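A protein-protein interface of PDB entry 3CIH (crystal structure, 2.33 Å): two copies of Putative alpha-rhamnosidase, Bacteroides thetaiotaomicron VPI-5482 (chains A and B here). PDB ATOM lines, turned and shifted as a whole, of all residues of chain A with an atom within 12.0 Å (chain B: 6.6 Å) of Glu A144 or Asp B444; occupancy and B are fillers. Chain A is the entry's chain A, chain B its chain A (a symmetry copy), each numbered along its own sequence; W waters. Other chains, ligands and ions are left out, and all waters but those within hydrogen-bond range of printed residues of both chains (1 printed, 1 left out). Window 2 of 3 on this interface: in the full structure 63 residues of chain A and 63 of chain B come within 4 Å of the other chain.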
ATOM      1  N   GLU A 140      16.919 -18.291   6.008  1.00  0.00           N
ATOM      2  CA  GLU A 140      16.619 -18.109   7.420  1.00  0.00           C
ATOM      3  C   GLU A 140      15.879 -19.297   8.022  1.00  0.00           C
ATOM      4  O   GLU A 140      14.787 -19.651   7.577  1.00  0.00           O
ATOM      5  CB  GLU A 140      15.797 -16.838   7.656  1.00  0.00           C
ATOM      6  CG  GLU A 140      15.646 -16.503   9.133  1.00  0.00           C
ATOM      7  CD  GLU A 140      14.978 -15.167   9.372  1.00  0.00           C
ATOM      8  OE1 GLU A 140      13.745 -15.078   9.193  1.00  0.00           O
ATOM      9  OE2 GLU A 140      15.691 -14.205   9.736  1.00  0.00           O
ATOM     10  N   TRP A 141      16.489 -19.906   9.037  1.00  0.00           N
ATOM     11  CA  TRP A 141      15.889 -21.041   9.730  1.00  0.00           C
ATOM     12  C   TRP A 141      15.944 -20.843  11.253  1.00  0.00           C
ATOM     13  O   TRP A 141      16.764 -20.074  11.765  1.00  0.00           O
ATOM     14  CB  TRP A 141      16.587 -22.352   9.337  1.00  0.00           C
ATOM     15  CG  TRP A 141      18.065 -22.375   9.571  1.00  0.00           C
ATOM     16  CD1 TRP A 141      19.037 -21.921   8.726  1.00  0.00           C
ATOM     17  CD2 TRP A 141      18.743 -22.877  10.730  1.00  0.00           C
ATOM     18  NE1 TRP A 141      20.276 -22.110   9.285  1.00  0.00           N
ATOM     19  CE2 TRP A 141      20.127 -22.694  10.516  1.00  0.00           C
ATOM     20  CE3 TRP A 141      18.313 -23.467  11.930  1.00  0.00           C
ATOM     21  CZ2 TRP A 141      21.092 -23.079  11.460  1.00  0.00           C
ATOM     22  CZ3 TRP A 141      19.271 -23.851  12.869  1.00  0.00           C
ATOM     23  CH2 TRP A 141      20.647 -23.653  12.625  1.00  0.00           C
ATOM     24  N   ILE A 142      15.070 -21.547  11.965  1.00  0.00           N
ATOM     25  CA  ILE A 142      14.994 -21.452  13.418  1.00  0.00           C
ATOM     26  C   ILE A 142      15.521 -22.727  14.082  1.00  0.00           C
ATOM     27  O   ILE A 142      15.125 -23.830  13.698  1.00  0.00           O
ATOM     28  CB  ILE A 142      13.531 -21.261  13.867  1.00  0.00           C
ATOM     29  CG1 ILE A 142      12.802 -20.339  12.887  1.00  0.00           C
ATOM     30  CG2 ILE A 142      13.489 -20.668  15.270  1.00  0.00           C
ATOM     31  CD1 ILE A 142      13.426 -18.948  12.771  1.00  0.00           C
ATOM     32  N   ASP A 143      16.406 -22.594  15.070  1.00  0.00           N
ATOM     33  CA  ASP A 143      16.905 -23.784  15.747  1.00  0.00           C
ATOM     34  C   ASP A 143      15.847 -24.245  16.754  1.00  0.00           C
ATOM     35  O   ASP A 143      14.837 -23.565  16.957  1.00  0.00           O
ATOM     36  CB  ASP A 143      18.253 -23.526  16.433  1.00  0.00           C
ATOM     37  CG  ASP A 143      18.165 -22.520  17.558  1.00  0.00           C
ATOM     38  OD1 ASP A 143      17.149 -22.508  18.281  1.00  0.00           O
ATOM     39  OD2 ASP A 143      19.132 -21.749  17.735  1.00  0.00           O
ATOM     40  N   GLU A 144      16.066 -25.382  17.399  1.00  0.00           N
ATOM     41  CA  GLU A 144      15.055 -25.898  18.309  1.00  0.00           C
ATOM     42  C   GLU A 144      14.730 -25.062  19.544  1.00  0.00           C
ATOM     43  O   GLU A 144      13.763 -25.359  20.236  1.00  0.00           O
ATOM     44  CB  GLU A 144      15.399 -27.328  18.721  1.00  0.00           C
ATOM     45  CG  GLU A 144      16.548 -27.455  19.677  1.00  0.00           C
ATOM     46  CD  GLU A 144      16.861 -28.896  19.980  1.00  0.00           C
ATOM     47  OE1 GLU A 144      15.929 -29.635  20.375  1.00  0.00           O
ATOM     48  OE2 GLU A 144      18.036 -29.292  19.826  1.00  0.00           O
ATOM     49  N   SER A 145      15.516 -24.024  19.819  1.00  0.00           N
ATOM     50  CA  SER A 145      15.255 -23.168  20.975  1.00  0.00           C
ATOM     51  C   SER A 145      14.399 -21.984  20.539  1.00  0.00           C
ATOM     52  O   SER A 145      13.784 -21.314  21.369  1.00  0.00           O
ATOM     53  CB  SER A 145      16.562 -22.632  21.567  1.00  0.00           C
ATOM     54  OG  SER A 145      17.033 -21.522  20.816  1.00  0.00           O
ATOM     55  N   GLY A 146      14.375 -21.724  19.236  1.00  0.00           N
ATOM     56  CA  GLY A 146      13.592 -20.619  18.708  1.00  0.00           C
ATOM     57  C   GLY A 146      14.443 -19.469  18.198  1.00  0.00           C
ATOM     58  O   GLY A 146      13.926 -18.422  17.819  1.00  0.00           O
ATOM     59  N   LYS A 147      15.756 -19.666  18.177  1.00  0.00           N
ATOM     60  CA  LYS A 147      16.690 -18.641  17.723  1.00  0.00           C
ATOM     61  C   LYS A 147      16.833 -18.647  16.203  1.00  0.00           C
ATOM     62  O   LYS A 147      17.032 -19.700  15.600  1.00  0.00           O
ATOM     63  CB  LYS A 147      18.053 -18.887  18.373  1.00  0.00           C
ATOM     64  CG  LYS A 147      19.100 -17.832  18.073  1.00  0.00           C
ATOM     65  CD  LYS A 147      20.461 -18.251  18.620  1.00  0.00           C
ATOM     66  CE  LYS A 147      21.477 -17.116  18.535  1.00  0.00           C
ATOM     67  NZ  LYS A 147      21.065 -15.930  19.359  1.00  0.00           N
ATOM     68  N   ALA A 148      16.739 -17.473  15.583  1.00  0.00           N
ATOM     69  CA  ALA A 148      16.855 -17.363  14.127  1.00  0.00           C
ATOM     70  C   ALA A 148      18.300 -17.475  13.669  1.00  0.00           C
ATOM     71  O   ALA A 148      19.216 -17.039  14.366  1.00  0.00           O
ATOM     72  CB  ALA A 148      16.260 -16.044  13.647  1.00  0.00           C
ATOM     73  N   SER A 149      18.498 -18.048  12.487  1.00  0.00           N
ATOM     74  CA  SER A 149      19.844 -18.230  11.958  1.00  0.00           C
ATOM     75  C   SER A 149      20.493 -16.923  11.534  1.00  0.00           C
ATOM     76  O   SER A 149      19.820 -15.906  11.355  1.00  0.00           O
ATOM     77  CB  SER A 149      19.829 -19.196  10.765  1.00  0.00           C
ATOM     78  OG  SER A 149      19.153 -18.634   9.647  1.00  0.00           O
ATOM     79  N   ASP A 150      21.813 -16.966  11.380  1.00  0.00           N
ATOM     80  CA  ASP A 150      22.589 -15.811  10.960  1.00  0.00           C
ATOM     81  C   ASP A 150      22.567 -15.738   9.437  1.00  0.00           C
ATOM     82  O   ASP A 150      23.212 -16.537   8.761  1.00  0.00           O
ATOM     83  CB  ASP A 150      24.028 -15.941  11.464  1.00  0.00           C
ATOM     84  CG  ASP A 150      24.937 -14.857  10.921  1.00  0.00           C
ATOM     85  OD1 ASP A 150      24.642 -13.658  11.113  1.00  0.00           O
ATOM     86  OD2 ASP A 150      25.956 -15.208  10.296  1.00  0.00           O
ATOM     87  N   ASP B 441      22.154 -33.283  14.412  1.00  0.00           N
ATOM     88  CA  ASP B 441      20.985 -33.712  15.164  1.00  0.00           C
ATOM     89  C   ASP B 441      20.463 -32.596  16.084  1.00  0.00           C
ATOM     90  O   ASP B 441      21.119 -31.562  16.257  1.00  0.00           O
ATOM     91  CB  ASP B 441      21.391 -34.940  15.981  1.00  0.00           C
ATOM     92  CG  ASP B 441      20.216 -35.663  16.594  1.00  0.00           C
ATOM     93  OD1 ASP B 441      19.058 -35.377  16.211  1.00  0.00           O
ATOM     94  OD2 ASP B 441      20.467 -36.533  17.457  1.00  0.00           O
ATOM     95  N   TRP B 442      19.273 -32.795  16.647  1.00  0.00           N
ATOM     96  CA  TRP B 442      18.704 -31.828  17.582  1.00  0.00           C
ATOM     97  C   TRP B 442      19.157 -32.342  18.944  1.00  0.00           C
ATOM     98  O   TRP B 442      18.442 -33.107  19.594  1.00  0.00           O
ATOM     99  CB  TRP B 442      17.169 -31.816  17.536  1.00  0.00           C
ATOM    100  CG  TRP B 442      16.556 -31.248  16.289  1.00  0.00           C
ATOM    101  CD1 TRP B 442      15.669 -31.874  15.461  1.00  0.00           C
ATOM    102  CD2 TRP B 442      16.728 -29.921  15.760  1.00  0.00           C
ATOM    103  NE1 TRP B 442      15.275 -31.023  14.455  1.00  0.00           N
ATOM    104  CE2 TRP B 442      15.908 -29.819  14.611  1.00  0.00           C
ATOM    105  CE3 TRP B 442      17.494 -28.810  16.144  1.00  0.00           C
ATOM    106  CZ2 TRP B 442      15.828 -28.653  13.843  1.00  0.00           C
ATOM    107  CZ3 TRP B 442      17.414 -27.644  15.379  1.00  0.00           C
ATOM    108  CH2 TRP B 442      16.582 -27.580  14.239  1.00  0.00           C
ATOM    109  N   ALA B 443      20.353 -31.933  19.360  1.00  0.00           N
ATOM    110  CA  ALA B 443      20.921 -32.372  20.630  1.00  0.00           C
ATOM    111  C   ALA B 443      20.945 -31.277  21.684  1.00  0.00           C
ATOM    112  O   ALA B 443      21.887 -31.168  22.459  1.00  0.00           O
ATOM    113  CB  ALA B 443      22.324 -32.914  20.409  1.00  0.00           C
ATOM    114  N   ASP B 444      19.902 -30.460  21.685  1.00  0.00           N
ATOM    115  CA  ASP B 444      19.728 -29.379  22.646  1.00  0.00           C
ATOM    116  C   ASP B 444      20.837 -28.343  22.752  1.00  0.00           C
ATOM    117  O   ASP B 444      20.914 -27.612  23.743  1.00  0.00           O
ATOM    118  CB  ASP B 444      19.440 -29.973  24.030  1.00  0.00           C
ATOM    119  CG  ASP B 444      18.184 -30.826  24.039  1.00  0.00           C
ATOM    120  OD1 ASP B 444      17.123 -30.308  23.631  1.00  0.00           O
ATOM    121  OD2 ASP B 444      18.255 -32.006  24.441  1.00  0.00           O
ATOM    122  N   GLY B 445      21.692 -28.268  21.740  1.00  0.00           N
ATOM    123  CA  GLY B 445      22.759 -27.280  21.756  1.00  0.00           C
ATOM    124  C   GLY B 445      24.074 -27.736  22.355  1.00  0.00           C
ATOM    125  O   GLY B 445      24.963 -26.924  22.574  1.00  0.00           O
ATOM    126  N   TYR B 446      24.209 -29.031  22.610  1.00  0.00           N
ATOM    127  CA  TYR B 446      25.430 -29.566  23.192  1.00  0.00           C
ATOM    128  C   TYR B 446      26.510 -29.908  22.174  1.00  0.00           C
ATOM    129  O   TYR B 446      27.650 -30.173  22.552  1.00  0.00           O
ATOM    130  CB  TYR B 446      25.108 -30.813  24.002  1.00  0.00           C
ATOM    131  CG  TYR B 446      24.514 -30.527  25.359  1.00  0.00           C
ATOM    132  CD1 TYR B 446      25.298 -29.993  26.380  1.00  0.00           C
ATOM    133  CD2 TYR B 446      23.171 -30.801  25.630  1.00  0.00           C
ATOM    134  CE1 TYR B 446      24.767 -29.740  27.643  1.00  0.00           C
ATOM    135  CE2 TYR B 446      22.626 -30.552  26.894  1.00  0.00           C
ATOM    136  CZ  TYR B 446      23.433 -30.024  27.895  1.00  0.00           C
ATOM    137  OH  TYR B 446      22.919 -29.805  29.151  1.00  0.00           O
ATOM    138  N   LEU B 447      26.160 -29.901  20.889  1.00  0.00           N
ATOM    139  CA  LEU B 447      27.111 -30.248  19.830  1.00  0.00           C
ATOM    140  C   LEU B 447      27.874 -29.084  19.193  1.00  0.00           C
ATOM    141  O   LEU B 447      27.274 -28.160  18.649  1.00  0.00           O
ATOM    142  CB  LEU B 447      26.393 -31.017  18.721  1.00  0.00           C
ATOM    143  CG  LEU B 447      25.709 -32.324  19.118  1.00  0.00           C
ATOM    144  CD1 LEU B 447      24.987 -32.896  17.912  1.00  0.00           C
ATOM    145  CD2 LEU B 447      26.733 -33.311  19.651  1.00  0.00           C
ATOM    146  N   THR B 555      17.998 -37.695  21.650  1.00  0.00           N
ATOM    147  CA  THR B 555      16.591 -37.450  21.966  1.00  0.00           C
ATOM    148  C   THR B 555      15.652 -37.284  20.767  1.00  0.00           C
ATOM    149  O   THR B 555      14.578 -36.693  20.890  1.00  0.00           O
ATOM    150  CB  THR B 555      16.430 -36.210  22.876  1.00  0.00           C
ATOM    151  OG1 THR B 555      17.082 -35.082  22.281  1.00  0.00           O
ATOM    152  CG2 THR B 555      17.026 -36.481  24.246  1.00  0.00           C
ATOM    153  N   THR B 556      16.052 -37.791  19.608  1.00  0.00           N
ATOM    154  CA  THR B 556      15.200 -37.712  18.424  1.00  0.00           C
ATOM    155  C   THR B 556      15.064 -39.113  17.870  1.00  0.00           C
ATOM    156  O   THR B 556      16.014 -39.892  17.911  1.00  0.00           O
ATOM    157  CB  THR B 556      15.798 -36.817  17.303  1.00  0.00           C
ATOM    158  OG1 THR B 556      17.051 -37.363  16.864  1.00  0.00           O
ATOM    159  CG2 THR B 556      16.005 -35.400  17.801  1.00  0.00           C
ATOM    160  N   LYS B 598      10.571 -35.247  17.914  1.00  0.00           N
ATOM    161  CA  LYS B 598      11.560 -35.339  18.981  1.00  0.00           C
ATOM    162  C   LYS B 598      10.901 -35.810  20.275  1.00  0.00           C
ATOM    163  O   LYS B 598       9.741 -35.500  20.542  1.00  0.00           O
ATOM    164  CB  LYS B 598      12.236 -33.980  19.217  1.00  0.00           C
ATOM    165  CG  LYS B 598      13.172 -33.983  20.407  1.00  0.00           C
ATOM    166  CD  LYS B 598      14.180 -32.856  20.381  1.00  0.00           C
ATOM    167  CE  LYS B 598      15.089 -32.949  21.606  1.00  0.00           C
ATOM    168  NZ  LYS B 598      16.176 -31.936  21.624  1.00  0.00           N
ATOM    169  N   ASN B 600      12.034 -36.622  24.517  1.00  0.00           N
ATOM    170  CA  ASN B 600      12.930 -36.751  25.651  1.00  0.00           C
ATOM    171  C   ASN B 600      12.092 -37.310  26.800  1.00  0.00           C
ATOM    172  O   ASN B 600      11.307 -36.585  27.413  1.00  0.00           O
ATOM    173  CB  ASN B 600      13.492 -35.385  26.046  1.00  0.00           C
ATOM    174  CG  ASN B 600      14.519 -35.483  27.161  1.00  0.00           C
ATOM    175  OD1 ASN B 600      14.526 -36.448  27.927  1.00  0.00           O
ATOM    176  ND2 ASN B 600      15.384 -34.477  27.262  1.00  0.00           N
ATOM    177  N   GLU B 603      11.194 -35.307  29.991  1.00  0.00           N
ATOM    178  CA  GLU B 603      10.186 -34.261  30.010  1.00  0.00           C
ATOM    179  C   GLU B 603       8.834 -34.882  30.337  1.00  0.00           C
ATOM    180  O   GLU B 603       8.698 -36.107  30.365  1.00  0.00           O
ATOM    181  CB  GLU B 603      10.138 -33.557  28.652  1.00  0.00           C
ATOM    182  CG  GLU B 603      11.445 -32.873  28.277  1.00  0.00           C
ATOM    183  CD  GLU B 603      11.364 -32.119  26.964  1.00  0.00           C
ATOM    184  OE1 GLU B 603      10.991 -32.739  25.946  1.00  0.00           O
ATOM    185  OE2 GLU B 603      11.676 -30.908  26.948  1.00  0.00           O
ATOM    186  N   ALA B 610       6.232 -28.660  22.955  1.00  0.00           N
ATOM    187  CA  ALA B 610       7.023 -27.503  22.572  1.00  0.00           C
ATOM    188  C   ALA B 610       8.309 -27.784  21.804  1.00  0.00           C
ATOM    189  O   ALA B 610       8.957 -28.817  21.970  1.00  0.00           O
ATOM    190  CB  ALA B 610       7.342 -26.663  23.810  1.00  0.00           C
ATOM    191  N   MET B 611       8.660 -26.826  20.957  1.00  0.00           N
ATOM    192  CA  MET B 611       9.875 -26.882  20.158  1.00  0.00           C
ATOM    193  C   MET B 611       9.987 -25.580  19.374  1.00  0.00           C
ATOM    194  O   MET B 611       8.987 -24.899  19.157  1.00  0.00           O
ATOM    195  CB  MET B 611       9.861 -28.083  19.206  1.00  0.00           C
ATOM    196  CG  MET B 611      11.212 -28.318  18.542  1.00  0.00           C
ATOM    197  SD  MET B 611      11.372 -30.106  17.767  1.00  0.00           S
ATOM    198  CE  MET B 611      13.363 -30.228  17.524  1.00  0.00           C
ATOM    199  N   TYR B 612      11.202 -25.239  18.953  1.00  0.00           N
ATOM    200  CA  TYR B 612      11.460 -24.002  18.213  1.00  0.00           C
ATOM    201  C   TYR B 612      10.995 -22.771  18.988  1.00  0.00           C
ATOM    202  O   TYR B 612      10.641 -21.746  18.401  1.00  0.00           O
ATOM    203  CB  TYR B 612      10.780 -24.049  16.842  1.00  0.00           C
ATOM    204  CG  TYR B 612      11.190 -25.247  16.038  1.00  0.00           C
ATOM    205  CD1 TYR B 612      12.480 -25.354  15.513  1.00  0.00           C
ATOM    206  CD2 TYR B 612      10.310 -26.315  15.854  1.00  0.00           C
ATOM    207  CE1 TYR B 612      12.885 -26.498  14.830  1.00  0.00           C
ATOM    208  CE2 TYR B 612      10.699 -27.460  15.176  1.00  0.00           C
ATOM    209  CZ  TYR B 612      11.990 -27.547  14.668  1.00  0.00           C
ATOM    210  OH  TYR B 612      12.394 -28.690  14.020  1.00  0.00           O
ATOM    211  N   GLY B 613      10.998 -22.884  20.315  1.00  0.00           N
ATOM    212  CA  GLY B 613      10.590 -21.780  21.165  1.00  0.00           C
ATOM    213  C   GLY B 613       9.103 -21.488  21.159  1.00  0.00           C
ATOM    214  O   GLY B 613       8.673 -20.435  21.621  1.00  0.00           O
ATOM    215  N   ARG B 614       8.311 -22.415  20.633  1.00  0.00           N
ATOM    216  CA  ARG B 614       6.861 -22.240  20.582  1.00  0.00           C
ATOM    217  C   ARG B 614       6.193 -23.380  21.345  1.00  0.00           C
ATOM    218  O   ARG B 614       6.633 -24.527  21.266  1.00  0.00           O
ATOM    219  CB  ARG B 614       6.381 -22.196  19.128  1.00  0.00           C
ATOM    220  CG  ARG B 614       6.986 -21.044  18.321  1.00  0.00           C
ATOM    221  CD  ARG B 614       6.164 -20.705  17.074  1.00  0.00           C
ATOM    222  NE  ARG B 614       6.745 -21.210  15.833  1.00  0.00           N
ATOM    223  CZ  ARG B 614       6.928 -22.495  15.562  1.00  0.00           C
ATOM    224  NH1 ARG B 614       6.577 -23.407  16.454  1.00  0.00           N
ATOM    225  NH2 ARG B 614       7.430 -22.870  14.395  1.00  0.00           N
HETATM  226  O   HOH W   1      20.240 -28.351  18.653  1.00  0.00           O
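Water W1 lies within hydrogen-bond range of the side-chain carboxylate (OE2) of Glu A144 (2.7 Å) and the backbone NH (N) of Gly B445 (3.4 Å).
No position is printed for both chains.
Of the 14 pairs that touch across the chains among the printed residues, none has its exchanged pair printed and touching as well.
Of the printed residues of chain B, Asp A143 touches Trp B442 and Tyr B612.
Glu A144 touches just these residues of chain B: Trp B442, Ala B443, Asp B444, Lys B598, Met B611, Tyr B612 and Gly B613.
Of the printed residues of chain B, Ser A145 touches Tyr B612 (3.8 Å) and Gly B613 (3.2 Å).
No residue of chain A comes within 4 Å of Asp B441.
Of chain A, only Asp A143 and Glu A144 come within 4 Å of Trp B442.
Ala B443 touches just one residue of chain A: Glu A144.
Of chain A, only Glu A144 comes within 4 Å of Asp B444.
No residue of chain A comes within 4 Å of Gly B445.
No residue of chain A comes within 4 Å of Tyr B446.
No residue of chain A comes within 4 Å of Leu B447.
No residue of chain A comes within 4 Å of Thr B555.
Met B611 touches one residue of chain A.
Of chain A, only Ile A142, Asp A143, Glu A144, Ser A145 and Gly A146 come within 4 Å of Tyr B612.
Gly B613 touches three residues of chain A.
The nearest residue of chain B that does not touch Glu A144 is Gly B445 (4.3 Å).
The nearest printed residue of chain B that does not touch Asp A143 is Gly B613 (5.1 Å).
The side-chain carboxylate (OE2) of Glu A144 lies within hydrogen-bond range of the backbone NH (N) of Asp B444.
OE1 of Glu A144 lies within salt-bridge range of NZ of Lys B598, at 2.6 Å.
The backbone carbonyl oxygen (O) of Glu A144 sits at hydrogen-bond distance from the backbone NH (N) of Tyr B612, 2.9 Å away.
The backbone NH (N) of Gly B613 lies close to the backbone carbonyl oxygen (O) of Ser A145, at 3.4 Å.
The side-chain carboxylate of Asp A143 sits at hydrogen-bond distance from the backbone NH of Ser A145 (2.7 Å).
The backbone NH (N) of Gly A146 lies within hydrogen-bond range of the side-chain carboxylate (OD1) of Asp A143.
The backbone NH (N) of Lys A147 lies within hydrogen-bond range of the side-chain carboxylate (OD1) of Asp A143, 3.2 Å away.
O of Trp B442 sits at hydrogen-bond distance from NZ of Lys B598, 3.3 Å away.
OD1 of Asp B444 lies within salt-bridge range of NZ of Lys B598 (2.8 Å).
OG1 of Thr B555 sits close to NZ of Lys B598 (3.3 Å).
Among the printed residues, merely in contact across the chains: Ile A142 with Tyr B612 (3.6 Å), Asp A143 with Trp B442 (3.9 Å), Asp A143 with Tyr B612 (3.3 Å), Glu A144 with Trp B442 (3.3 Å), Glu A144 with Ala B443 (3.5 Å), Glu A144 with Met B611 (3.7 Å), Glu A144 with Gly B613 (3.7 Å), Ser A145 with Tyr B612 (3.8 Å), Gly A146 with Tyr B612 (3.2 Å) and Gly A146 with Gly B613 (3.7 Å).
Of the 17 printed residues of chain B, 7 touch a printed residue of chain A.
Printed residues of chain B that touch a printed residue of chain A: Trp B442, Ala B443, Asp B444, Lys B598, Met B611, Tyr B612 and Gly B613.
Hydrophobic or aromatic side chains of chain B within 4 Å of the printed part of chain A: Trp B442, Met B611 and Tyr B612.
Printed residues of chain A that touch a printed residue of chain B: Ile A142, Asp A143, Glu A144, Ser A145 and Gly A146.
Among the printed residues, 14 pairs touch across the chains.
Among the printed residues, Asp or Glu carboxylates within 4 Å of a Lys or Arg side-chain nitrogen of the other chain: Glu A144 with Lys B598 (2.6 Å).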
